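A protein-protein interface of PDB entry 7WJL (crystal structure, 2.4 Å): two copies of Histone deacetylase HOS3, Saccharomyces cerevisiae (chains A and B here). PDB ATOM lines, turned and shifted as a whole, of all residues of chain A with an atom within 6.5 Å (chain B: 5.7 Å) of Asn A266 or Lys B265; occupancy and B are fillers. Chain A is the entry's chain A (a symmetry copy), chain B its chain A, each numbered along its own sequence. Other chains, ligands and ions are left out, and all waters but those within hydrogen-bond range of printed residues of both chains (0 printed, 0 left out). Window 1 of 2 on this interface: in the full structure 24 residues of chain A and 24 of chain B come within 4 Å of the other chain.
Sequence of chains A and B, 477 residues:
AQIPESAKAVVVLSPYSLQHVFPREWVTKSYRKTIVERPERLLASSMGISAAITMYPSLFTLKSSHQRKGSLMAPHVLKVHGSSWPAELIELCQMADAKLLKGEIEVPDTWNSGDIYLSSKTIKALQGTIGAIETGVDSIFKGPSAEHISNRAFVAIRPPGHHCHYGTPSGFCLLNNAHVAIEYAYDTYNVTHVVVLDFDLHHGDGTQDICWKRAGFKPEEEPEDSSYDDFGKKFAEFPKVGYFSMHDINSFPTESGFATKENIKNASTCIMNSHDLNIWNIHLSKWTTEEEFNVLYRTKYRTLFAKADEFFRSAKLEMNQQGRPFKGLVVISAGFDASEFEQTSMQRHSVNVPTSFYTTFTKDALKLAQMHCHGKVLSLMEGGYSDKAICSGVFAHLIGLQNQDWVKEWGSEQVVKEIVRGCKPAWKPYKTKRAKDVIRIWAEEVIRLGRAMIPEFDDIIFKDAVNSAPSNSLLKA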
ATOM      1  N   HIS A 165     -27.185  -0.212   5.220  1.00  0.00           N
ATOM      2  CA  HIS A 165     -26.472   0.805   4.476  1.00  0.00           C
ATOM      3  C   HIS A 165     -25.860   0.194   3.221  1.00  0.00           C
ATOM      4  O   HIS A 165     -26.057  -0.981   2.903  1.00  0.00           O
ATOM      5  CB  HIS A 165     -25.390   1.430   5.362  1.00  0.00           C
ATOM      6  CG  HIS A 165     -25.929   2.323   6.439  1.00  0.00           C
ATOM      7  ND1 HIS A 165     -26.896   1.909   7.336  1.00  0.00           N
ATOM      8  CD2 HIS A 165     -25.632   3.605   6.774  1.00  0.00           C
ATOM      9  CE1 HIS A 165     -27.169   2.895   8.176  1.00  0.00           C
ATOM     10  NE2 HIS A 165     -26.418   3.935   7.855  1.00  0.00           N
ATOM     11  N   HIS A 203     -36.208   6.366  11.060  1.00  0.00           N
ATOM     12  CA  HIS A 203     -35.570   6.877   9.857  1.00  0.00           C
ATOM     13  C   HIS A 203     -34.965   5.723   9.050  1.00  0.00           C
ATOM     14  O   HIS A 203     -34.308   4.840   9.604  1.00  0.00           O
ATOM     15  CB  HIS A 203     -34.497   7.890  10.230  1.00  0.00           C
ATOM     16  CG  HIS A 203     -33.724   8.398   9.058  1.00  0.00           C
ATOM     17  ND1 HIS A 203     -32.352   8.537   9.074  1.00  0.00           N
ATOM     18  CD2 HIS A 203     -34.130   8.798   7.826  1.00  0.00           C
ATOM     19  CE1 HIS A 203     -31.945   9.004   7.906  1.00  0.00           C
ATOM     20  NE2 HIS A 203     -33.005   9.176   7.133  1.00  0.00           N
ATOM     21  N   ASP A 205     -32.275   5.182   7.546  1.00  0.00           N
ATOM     22  CA  ASP A 205     -30.914   5.671   7.335  1.00  0.00           C
ATOM     23  C   ASP A 205     -30.159   4.832   6.306  1.00  0.00           C
ATOM     24  O   ASP A 205     -29.250   5.341   5.641  1.00  0.00           O
ATOM     25  CB  ASP A 205     -30.146   5.707   8.665  1.00  0.00           C
ATOM     26  CG  ASP A 205     -30.146   4.354   9.402  1.00  0.00           C
ATOM     27  OD1 ASP A 205     -30.990   3.477   9.122  1.00  0.00           O
ATOM     28  OD2 ASP A 205     -29.300   4.174  10.294  1.00  0.00           O
ATOM     29  N   GLN A 208     -31.466   5.844   2.809  1.00  0.00           N
ATOM     30  CA  GLN A 208     -30.971   7.175   2.483  1.00  0.00           C
ATOM     31  C   GLN A 208     -29.473   7.149   2.191  1.00  0.00           C
ATOM     32  O   GLN A 208     -29.002   7.806   1.257  1.00  0.00           O
ATOM     33  CB  GLN A 208     -31.284   8.138   3.623  1.00  0.00           C
ATOM     34  CG  GLN A 208     -30.927   9.598   3.300  1.00  0.00           C
ATOM     35  CD  GLN A 208     -31.371  10.545   4.392  1.00  0.00           C
ATOM     36  OE1 GLN A 208     -32.548  10.541   4.775  1.00  0.00           O
ATOM     37  NE2 GLN A 208     -30.436  11.351   4.917  1.00  0.00           N
ATOM     38  N   ASP A 209     -28.712   6.411   2.997  1.00  0.00           N
ATOM     39  CA  ASP A 209     -27.292   6.226   2.742  1.00  0.00           C
ATOM     40  C   ASP A 209     -27.043   5.765   1.303  1.00  0.00           C
ATOM     41  O   ASP A 209     -26.125   6.249   0.629  1.00  0.00           O
ATOM     42  CB  ASP A 209     -26.733   5.218   3.750  1.00  0.00           C
ATOM     43  CG  ASP A 209     -25.259   4.917   3.522  1.00  0.00           C
ATOM     44  OD1 ASP A 209     -24.427   5.704   4.022  1.00  0.00           O
ATOM     45  OD2 ASP A 209     -24.933   3.896   2.855  1.00  0.00           O
ATOM     46  N   TRP A 212     -27.286   8.471  -1.230  1.00  0.00           N
ATOM     47  CA  TRP A 212     -26.051   9.232  -1.391  1.00  0.00           C
ATOM     48  C   TRP A 212     -25.099   8.525  -2.347  1.00  0.00           C
ATOM     49  O   TRP A 212     -24.435   9.177  -3.161  1.00  0.00           O
ATOM     50  CB  TRP A 212     -25.377   9.467  -0.030  1.00  0.00           C
ATOM     51  CG  TRP A 212     -25.957  10.611   0.742  1.00  0.00           C
ATOM     52  CD1 TRP A 212     -26.948  10.544   1.674  1.00  0.00           C
ATOM     53  CD2 TRP A 212     -25.579  11.992   0.659  1.00  0.00           C
ATOM     54  NE1 TRP A 212     -27.211  11.789   2.176  1.00  0.00           N
ATOM     55  CE2 TRP A 212     -26.381  12.700   1.576  1.00  0.00           C
ATOM     56  CE3 TRP A 212     -24.630  12.697  -0.090  1.00  0.00           C
ATOM     57  CZ2 TRP A 212     -26.274  14.083   1.762  1.00  0.00           C
ATOM     58  CZ3 TRP A 212     -24.527  14.077   0.094  1.00  0.00           C
ATOM     59  CH2 TRP A 212     -25.347  14.750   1.017  1.00  0.00           C
ATOM     60  N   GLU A 220     -18.818   5.679   2.901  1.00  0.00           N
ATOM     61  CA  GLU A 220     -17.824   5.620   3.969  1.00  0.00           C
ATOM     62  C   GLU A 220     -17.059   4.298   3.932  1.00  0.00           C
ATOM     63  O   GLU A 220     -15.857   4.261   4.222  1.00  0.00           O
ATOM     64  CB  GLU A 220     -18.506   5.819   5.327  1.00  0.00           C
ATOM     65  CG  GLU A 220     -19.817   5.035   5.462  1.00  0.00           C
ATOM     66  CD  GLU A 220     -20.691   5.469   6.638  1.00  0.00           C
ATOM     67  OE1 GLU A 220     -20.295   5.228   7.800  1.00  0.00           O
ATOM     68  OE2 GLU A 220     -21.792   6.017   6.396  1.00  0.00           O
ATOM     69  N   HIS A 247     -40.812  10.185  10.375  1.00  0.00           N
ATOM     70  CA  HIS A 247     -40.291   9.293  11.398  1.00  0.00           C
ATOM     71  C   HIS A 247     -40.123  10.078  12.689  1.00  0.00           C
ATOM     72  O   HIS A 247     -40.167  11.311  12.699  1.00  0.00           O
ATOM     73  CB  HIS A 247     -38.961   8.666  10.951  1.00  0.00           C
ATOM     74  CG  HIS A 247     -37.916   9.681  10.594  1.00  0.00           C
ATOM     75  ND1 HIS A 247     -37.728  10.134   9.306  1.00  0.00           N
ATOM     76  CD2 HIS A 247     -37.033  10.364  11.366  1.00  0.00           C
ATOM     77  CE1 HIS A 247     -36.763  11.042   9.296  1.00  0.00           C
ATOM     78  NE2 HIS A 247     -36.323  11.197  10.532  1.00  0.00           N
ATOM     79  N   LYS A 261     -24.245  13.051  16.298  1.00  0.00           N
ATOM     80  CA  LYS A 261     -24.255  14.157  15.350  1.00  0.00           C
ATOM     81  C   LYS A 261     -24.582  13.656  13.946  1.00  0.00           C
ATOM     82  O   LYS A 261     -25.537  14.111  13.301  1.00  0.00           O
ATOM     83  CB  LYS A 261     -22.874  14.857  15.421  1.00  0.00           C
ATOM     84  CG  LYS A 261     -22.590  15.998  14.443  1.00  0.00           C
ATOM     85  CD  LYS A 261     -21.144  16.607  14.597  1.00  0.00           C
ATOM     86  CE  LYS A 261     -21.073  17.747  15.644  1.00  0.00           C
ATOM     87  NZ  LYS A 261     -19.779  18.556  15.765  1.00  0.00           N
ATOM     88  N   GLU A 262     -23.823  12.667  13.484  1.00  0.00           N
ATOM     89  CA  GLU A 262     -23.940  12.252  12.094  1.00  0.00           C
ATOM     90  C   GLU A 262     -25.316  11.654  11.805  1.00  0.00           C
ATOM     91  O   GLU A 262     -25.915  11.934  10.760  1.00  0.00           O
ATOM     92  CB  GLU A 262     -22.824  11.261  11.744  1.00  0.00           C
ATOM     93  CG  GLU A 262     -22.780  10.876  10.265  1.00  0.00           C
ATOM     94  CD  GLU A 262     -22.842  12.081   9.307  1.00  0.00           C
ATOM     95  OE1 GLU A 262     -22.100  13.080   9.508  1.00  0.00           O
ATOM     96  OE2 GLU A 262     -23.638  12.020   8.344  1.00  0.00           O
ATOM     97  N   ASN A 263     -25.842  10.840  12.718  1.00  0.00           N
ATOM     98  CA  ASN A 263     -27.146  10.236  12.456  1.00  0.00           C
ATOM     99  C   ASN A 263     -28.278  11.241  12.614  1.00  0.00           C
ATOM    100  O   ASN A 263     -29.287  11.149  11.900  1.00  0.00           O
ATOM    101  CB  ASN A 263     -27.353   9.028  13.369  1.00  0.00           C
ATOM    102  CG  ASN A 263     -26.445   7.870  12.990  1.00  0.00           C
ATOM    103  OD1 ASN A 263     -26.040   7.746  11.835  1.00  0.00           O
ATOM    104  ND2 ASN A 263     -26.115   7.029  13.957  1.00  0.00           N
ATOM    105  N   ILE A 264     -28.131  12.199  13.535  1.00  0.00           N
ATOM    106  CA  ILE A 264     -29.114  13.266  13.653  1.00  0.00           C
ATOM    107  C   ILE A 264     -29.178  14.059  12.351  1.00  0.00           C
ATOM    108  O   ILE A 264     -30.265  14.370  11.859  1.00  0.00           O
ATOM    109  CB  ILE A 264     -28.790  14.167  14.866  1.00  0.00           C
ATOM    110  CG1 ILE A 264     -28.942  13.383  16.183  1.00  0.00           C
ATOM    111  CG2 ILE A 264     -29.679  15.388  14.877  1.00  0.00           C
ATOM    112  CD1 ILE A 264     -28.221  14.005  17.375  1.00  0.00           C
ATOM    113  N   LYS A 265     -28.013  14.385  11.772  1.00  0.00           N
ATOM    114  CA  LYS A 265     -27.975  15.127  10.507  1.00  0.00           C
ATOM    115  C   LYS A 265     -28.684  14.371   9.389  1.00  0.00           C
ATOM    116  O   LYS A 265     -29.467  14.951   8.628  1.00  0.00           O
ATOM    117  CB  LYS A 265     -26.531  15.405  10.069  1.00  0.00           C
ATOM    118  CG  LYS A 265     -25.795  16.427  10.880  1.00  0.00           C
ATOM    119  CD  LYS A 265     -24.355  16.528  10.419  1.00  0.00           C
ATOM    120  CE  LYS A 265     -23.576  17.404  11.349  1.00  0.00           C
ATOM    121  NZ  LYS A 265     -22.159  17.518  10.914  1.00  0.00           N
ATOM    122  N   ASN A 266     -28.388  13.080   9.240  1.00  0.00           N
ATOM    123  CA  ASN A 266     -29.013  12.353   8.145  1.00  0.00           C
ATOM    124  C   ASN A 266     -30.516  12.254   8.356  1.00  0.00           C
ATOM    125  O   ASN A 266     -31.300  12.364   7.401  1.00  0.00           O
ATOM    126  CB  ASN A 266     -28.370  10.979   7.999  1.00  0.00           C
ATOM    127  CG  ASN A 266     -26.896  11.074   7.635  1.00  0.00           C
ATOM    128  OD1 ASN A 266     -26.488  12.036   6.989  1.00  0.00           O
ATOM    129  ND2 ASN A 266     -26.095  10.105   8.068  1.00  0.00           N
ATOM    130  N   ALA A 267     -30.935  12.065   9.598  1.00  0.00           N
ATOM    131  CA  ALA A 267     -32.359  11.953   9.859  1.00  0.00           C
ATOM    132  C   ALA A 267     -33.085  13.292   9.746  1.00  0.00           C
ATOM    133  O   ALA A 267     -34.313  13.306   9.879  1.00  0.00           O
ATOM    134  CB  ALA A 267     -32.588  11.339  11.246  1.00  0.00           C
ATOM    135  N   SER A 268     -32.374  14.404   9.505  1.00  0.00           N
ATOM    136  CA  SER A 268     -33.005  15.713   9.370  1.00  0.00           C
ATOM    137  C   SER A 268     -32.779  16.348   8.000  1.00  0.00           C
ATOM    138  O   SER A 268     -33.041  17.548   7.838  1.00  0.00           O
ATOM    139  CB  SER A 268     -32.521  16.669  10.469  1.00  0.00           C
ATOM    140  OG  SER A 268     -32.511  16.062  11.754  1.00  0.00           O
ATOM    141  N   THR A 269     -32.311  15.584   7.008  1.00  0.00           N
ATOM    142  CA  THR A 269     -31.911  16.164   5.730  1.00  0.00           C
ATOM    143  C   THR A 269     -33.117  16.499   4.851  1.00  0.00           C
ATOM    144  O   THR A 269     -33.969  15.638   4.592  1.00  0.00           O
ATOM    145  CB  THR A 269     -30.970  15.209   4.988  1.00  0.00           C
ATOM    146  OG1 THR A 269     -29.757  15.056   5.741  1.00  0.00           O
ATOM    147  CG2 THR A 269     -30.614  15.753   3.595  1.00  0.00           C
ATOM    148  N   CYS A 270     -33.183  17.750   4.384  1.00  0.00           N
ATOM    149  CA  CYS A 270     -34.187  18.170   3.401  1.00  0.00           C
ATOM    150  C   CYS A 270     -33.524  18.897   2.237  1.00  0.00           C
ATOM    151  O   CYS A 270     -33.020  20.014   2.396  1.00  0.00           O
ATOM    152  CB  CYS A 270     -35.281  19.039   4.019  1.00  0.00           C
ATOM    153  SG  CYS A 270     -36.262  18.150   5.278  1.00  0.00           S
ATOM    154  N   ILE A 279     -33.968  14.191  -1.185  1.00  0.00           N
ATOM    155  CA  ILE A 279     -34.109  13.617   0.148  1.00  0.00           C
ATOM    156  C   ILE A 279     -34.952  14.566   0.988  1.00  0.00           C
ATOM    157  O   ILE A 279     -34.684  15.773   1.027  1.00  0.00           O
ATOM    158  CB  ILE A 279     -32.739  13.385   0.808  1.00  0.00           C
ATOM    159  CG1 ILE A 279     -31.928  12.384  -0.008  1.00  0.00           C
ATOM    160  CG2 ILE A 279     -32.886  12.949   2.267  1.00  0.00           C
ATOM    161  CD1 ILE A 279     -30.458  12.360   0.367  1.00  0.00           C
ATOM    162  N   ASN A 281     -36.961  14.606   4.878  1.00  0.00           N
ATOM    163  CA  ASN A 281     -37.201  13.961   6.162  1.00  0.00           C
ATOM    164  C   ASN A 281     -38.059  14.872   7.023  1.00  0.00           C
ATOM    165  O   ASN A 281     -37.712  16.035   7.215  1.00  0.00           O
ATOM    166  CB  ASN A 281     -35.887  13.678   6.896  1.00  0.00           C
ATOM    167  CG  ASN A 281     -35.138  12.524   6.304  1.00  0.00           C
ATOM    168  OD1 ASN A 281     -35.580  11.376   6.394  1.00  0.00           O
ATOM    169  ND2 ASN A 281     -33.998  12.810   5.686  1.00  0.00           N
ATOM    170  N   GLN B 208     -24.153  27.837  12.337  1.00  0.00           N
ATOM    171  CA  GLN B 208     -24.813  26.573  12.635  1.00  0.00           C
ATOM    172  C   GLN B 208     -23.862  25.607  13.337  1.00  0.00           C
ATOM    173  O   GLN B 208     -24.251  24.918  14.284  1.00  0.00           O
ATOM    174  CB  GLN B 208     -25.359  25.958  11.351  1.00  0.00           C
ATOM    175  CG  GLN B 208     -26.200  24.694  11.593  1.00  0.00           C
ATOM    176  CD  GLN B 208     -26.838  24.186  10.320  1.00  0.00           C
ATOM    177  OE1 GLN B 208     -27.526  24.944   9.625  1.00  0.00           O
ATOM    178  NE2 GLN B 208     -26.605  22.906   9.991  1.00  0.00           N
ATOM    179  N   THR B 260     -19.172  19.214  -0.754  1.00  0.00           N
ATOM    180  CA  THR B 260     -18.952  17.966  -0.043  1.00  0.00           C
ATOM    181  C   THR B 260     -20.238  17.500   0.618  1.00  0.00           C
ATOM    182  O   THR B 260     -21.089  18.306   1.023  1.00  0.00           O
ATOM    183  CB  THR B 260     -17.857  18.092   1.015  1.00  0.00           C
ATOM    184  OG1 THR B 260     -18.279  19.007   2.033  1.00  0.00           O
ATOM    185  CG2 THR B 260     -16.578  18.582   0.398  1.00  0.00           C
ATOM    186  N   LYS B 261     -20.369  16.172   0.689  1.00  0.00           N
ATOM    187  CA  LYS B 261     -21.393  15.486   1.464  1.00  0.00           C
ATOM    188  C   LYS B 261     -21.669  16.231   2.767  1.00  0.00           C
ATOM    189  O   LYS B 261     -22.806  16.624   3.062  1.00  0.00           O
ATOM    190  CB  LYS B 261     -20.913  14.032   1.704  1.00  0.00           C
ATOM    191  CG  LYS B 261     -21.770  13.123   2.586  1.00  0.00           C
ATOM    192  CD  LYS B 261     -21.161  11.682   2.776  1.00  0.00           C
ATOM    193  CE  LYS B 261     -21.593  10.688   1.669  1.00  0.00           C
ATOM    194  NZ  LYS B 261     -21.233   9.209   1.825  1.00  0.00           N
ATOM    195  N   GLU B 262     -20.612  16.485   3.533  1.00  0.00           N
ATOM    196  CA  GLU B 262     -20.799  17.023   4.872  1.00  0.00           C
ATOM    197  C   GLU B 262     -21.407  18.424   4.829  1.00  0.00           C
ATOM    198  O   GLU B 262     -22.296  18.747   5.626  1.00  0.00           O
ATOM    199  CB  GLU B 262     -19.468  17.023   5.631  1.00  0.00           C
ATOM    200  CG  GLU B 262     -19.591  17.440   7.097  1.00  0.00           C
ATOM    201  CD  GLU B 262     -20.721  16.718   7.856  1.00  0.00           C
ATOM    202  OE1 GLU B 262     -20.841  15.466   7.759  1.00  0.00           O
ATOM    203  OE2 GLU B 262     -21.490  17.413   8.557  1.00  0.00           O
ATOM    204  N   ASN B 263     -20.954  19.268   3.904  1.00  0.00           N
ATOM    205  CA  ASN B 263     -21.501  20.622   3.856  1.00  0.00           C
ATOM    206  C   ASN B 263     -22.906  20.644   3.274  1.00  0.00           C
ATOM    207  O   ASN B 263     -23.729  21.478   3.681  1.00  0.00           O
ATOM    208  CB  ASN B 263     -20.563  21.534   3.066  1.00  0.00           C
ATOM    209  CG  ASN B 263     -19.269  21.799   3.813  1.00  0.00           C
ATOM    210  OD1 ASN B 263     -19.233  21.745   5.041  1.00  0.00           O
ATOM    211  ND2 ASN B 263     -18.201  22.075   3.080  1.00  0.00           N
ATOM    212  N   ILE B 264     -23.199  19.746   2.329  1.00  0.00           N
ATOM    213  CA  ILE B 264     -24.558  19.627   1.818  1.00  0.00           C
ATOM    214  C   ILE B 264     -25.505  19.243   2.951  1.00  0.00           C
ATOM    215  O   ILE B 264     -26.592  19.813   3.080  1.00  0.00           O
ATOM    216  CB  ILE B 264     -24.610  18.616   0.651  1.00  0.00           C
ATOM    217  CG1 ILE B 264     -23.810  19.137  -0.558  1.00  0.00           C
ATOM    218  CG2 ILE B 264     -26.039  18.333   0.252  1.00  0.00           C
ATOM    219  CD1 ILE B 264     -23.410  18.061  -1.562  1.00  0.00           C
ATOM    220  N   LYS B 265     -25.100  18.281   3.793  1.00  0.00           N
ATOM    221  CA  LYS B 265     -25.933  17.861   4.925  1.00  0.00           C
ATOM    222  C   LYS B 265     -26.213  19.018   5.877  1.00  0.00           C
ATOM    223  O   LYS B 265     -27.353  19.217   6.317  1.00  0.00           O
ATOM    224  CB  LYS B 265     -25.267  16.728   5.716  1.00  0.00           C
ATOM    225  CG  LYS B 265     -25.235  15.396   5.033  1.00  0.00           C
ATOM    226  CD  LYS B 265     -24.456  14.396   5.865  1.00  0.00           C
ATOM    227  CE  LYS B 265     -24.263  13.127   5.098  1.00  0.00           C
ATOM    228  NZ  LYS B 265     -23.502  12.131   5.898  1.00  0.00           N
ATOM    229  N   ASN B 266     -25.179  19.770   6.249  1.00  0.00           N
ATOM    230  CA  ASN B 266     -25.415  20.846   7.200  1.00  0.00           C
ATOM    231  C   ASN B 266     -26.308  21.915   6.588  1.00  0.00           C
ATOM    232  O   ASN B 266     -27.182  22.477   7.266  1.00  0.00           O
ATOM    233  CB  ASN B 266     -24.087  21.422   7.676  1.00  0.00           C
ATOM    234  CG  ASN B 266     -23.254  20.392   8.425  1.00  0.00           C
ATOM    235  OD1 ASN B 266     -23.813  19.492   9.046  1.00  0.00           O
ATOM    236  ND2 ASN B 266     -21.931  20.501   8.348  1.00  0.00           N
ATOM    237  N   ALA B 267     -26.114  22.196   5.308  1.00  0.00           N
ATOM    238  CA  ALA B 267     -26.930  23.215   4.672  1.00  0.00           C
ATOM    239  C   ALA B 267     -28.364  22.751   4.424  1.00  0.00           C
ATOM    240  O   ALA B 267     -29.168  23.560   3.951  1.00  0.00           O
ATOM    241  CB  ALA B 267     -26.279  23.657   3.356  1.00  0.00           C
ATOM    242  N   SER B 268     -28.705  21.489   4.727  1.00  0.00           N
ATOM    243  CA  SER B 268     -30.060  20.984   4.530  1.00  0.00           C
ATOM    244  C   SER B 268     -30.724  20.526   5.826  1.00  0.00           C
ATOM    245  O   SER B 268     -31.761  19.853   5.771  1.00  0.00           O
ATOM    246  CB  SER B 268     -30.073  19.838   3.509  1.00  0.00           C
ATOM    247  OG  SER B 268     -29.294  20.125   2.357  1.00  0.00           O
ATOM    248  N   THR B 269     -30.165  20.874   6.990  1.00  0.00           N
ATOM    249  CA  THR B 269     -30.647  20.328   8.254  1.00  0.00           C
ATOM    250  C   THR B 269     -31.939  21.005   8.715  1.00  0.00           C
ATOM    251  O   THR B 269     -32.003  22.237   8.822  1.00  0.00           O
ATOM    252  CB  THR B 269     -29.569  20.466   9.335  1.00  0.00           C
ATOM    253  OG1 THR B 269     -28.431  19.666   8.975  1.00  0.00           O
ATOM    254  CG2 THR B 269     -30.088  19.987  10.700  1.00  0.00           C
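The side-chain carboxylate (OE1) of Glu A262 lies close to the side-chain carboxylate (OE1) of Glu B262 (3.2 Å).
NZ of Lys A265 lies within salt-bridge range of OE2 of Glu B262.
O of Ser B268 lies within hydrogen-bond range of N of Cys A270 (2.9 Å).
The backbone carbonyl oxygen of Ser A268 sits close to the backbone carbonyl oxygen of Ser B268.
OD1 of Asn B266 lies close to NZ of Lys A265, 3.2 Å away.
The side-chain amino group of Lys B265 lies close to the side-chain amide oxygen of Asn A266.
OE2 of Glu A262 lies within salt-bridge range of NZ of Lys B265 (2.5 Å).
O of Asn A281 is in hydrogen-bond range of SG of Cys A270 (3.2 Å).
The side-chain carboxylate (OE2) of Glu B262 lies within hydrogen-bond range of the side-chain amide nitrogen (ND2) of Asn B266 (3.1 Å).
ND2 of Asn A266 sits at hydrogen-bond distance from OE2 of Glu A262 (3.1 Å).
The side-chain amide nitrogen (NE2) of Gln A208 lies within hydrogen-bond range of the backbone carbonyl oxygen (O) of Asn A266.
The side-chain hydroxyl (OG1) of Thr A269 is in hydrogen-bond range of the backbone carbonyl oxygen (O) of Lys A265 (2.9 Å).
The backbone carbonyl oxygen of Ile A264 lies within hydrogen-bond range of the side-chain hydroxyl of Ser A268, 2.8 Å away.
Among the printed residues, pairs that only touch across the chains: Trp A212 with Lys B265, Ser A268 with Thr B269, Thr A269 with Ser B268, Trp A212 with Lys B261 and Trp A212 with Ile B264.
Printed residues of chain B within 4 Å of Asn A266: Lys B265.
Of the printed residues of chain A, Lys B265 touches Trp A212, Glu A262 and Asn A266.
Of the printed residues of chain A, Ser B268 touches Ser A268 (3.4 Å), Thr A269 (3.7 Å) and Cys A270 (2.9 Å).
Of the printed residues of chain B, Trp A212 touches Lys B261 (3.7 Å), Ile B264 (3.7 Å) and Lys B265 (3.7 Å).
Printed residues of chain A within 4 Å of Glu B262: Glu A262 and Lys A265.
Printed residues of chain B within 4 Å of Ser A268: Ser B268 (3.4 Å) and Thr B269 (3.7 Å).
The nearest printed residue of chain A that does not touch Ser B268 is Lys A265 (6.1 Å).
Of the 11 printed residues of chain B, 7 touch a printed residue of chain A.
Of the 20 printed residues of chain A, 7 touch a printed residue of chain B.
Among the printed residues, 12 pairs touch across the chains.
Among the printed residues, Asp or Glu carboxylates within 4 Å of a Lys or Arg side-chain nitrogen of the other chain: Glu A262 with Lys B265 and Lys A265 with Glu B262.
Glu B262 touches its own counterpart, Glu A262.
Glu A262 touches Lys B265, and with the chains exchanged Lys A265 touches Glu B262.
Lys A265 touches Asn B266, and with the chains exchanged Asn A266 touches Lys B265.
Ser A268 touches Thr B269, and with the chains exchanged Thr A269 touches Ser B268.
Positions printed for both chains: 208, 261, 262, 263, 264, 265, 266, 267, 268 and 269.
Of the 12 pairs that touch across the chains among the printed residues, 8 have their exchanged pair printed and touching as well.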
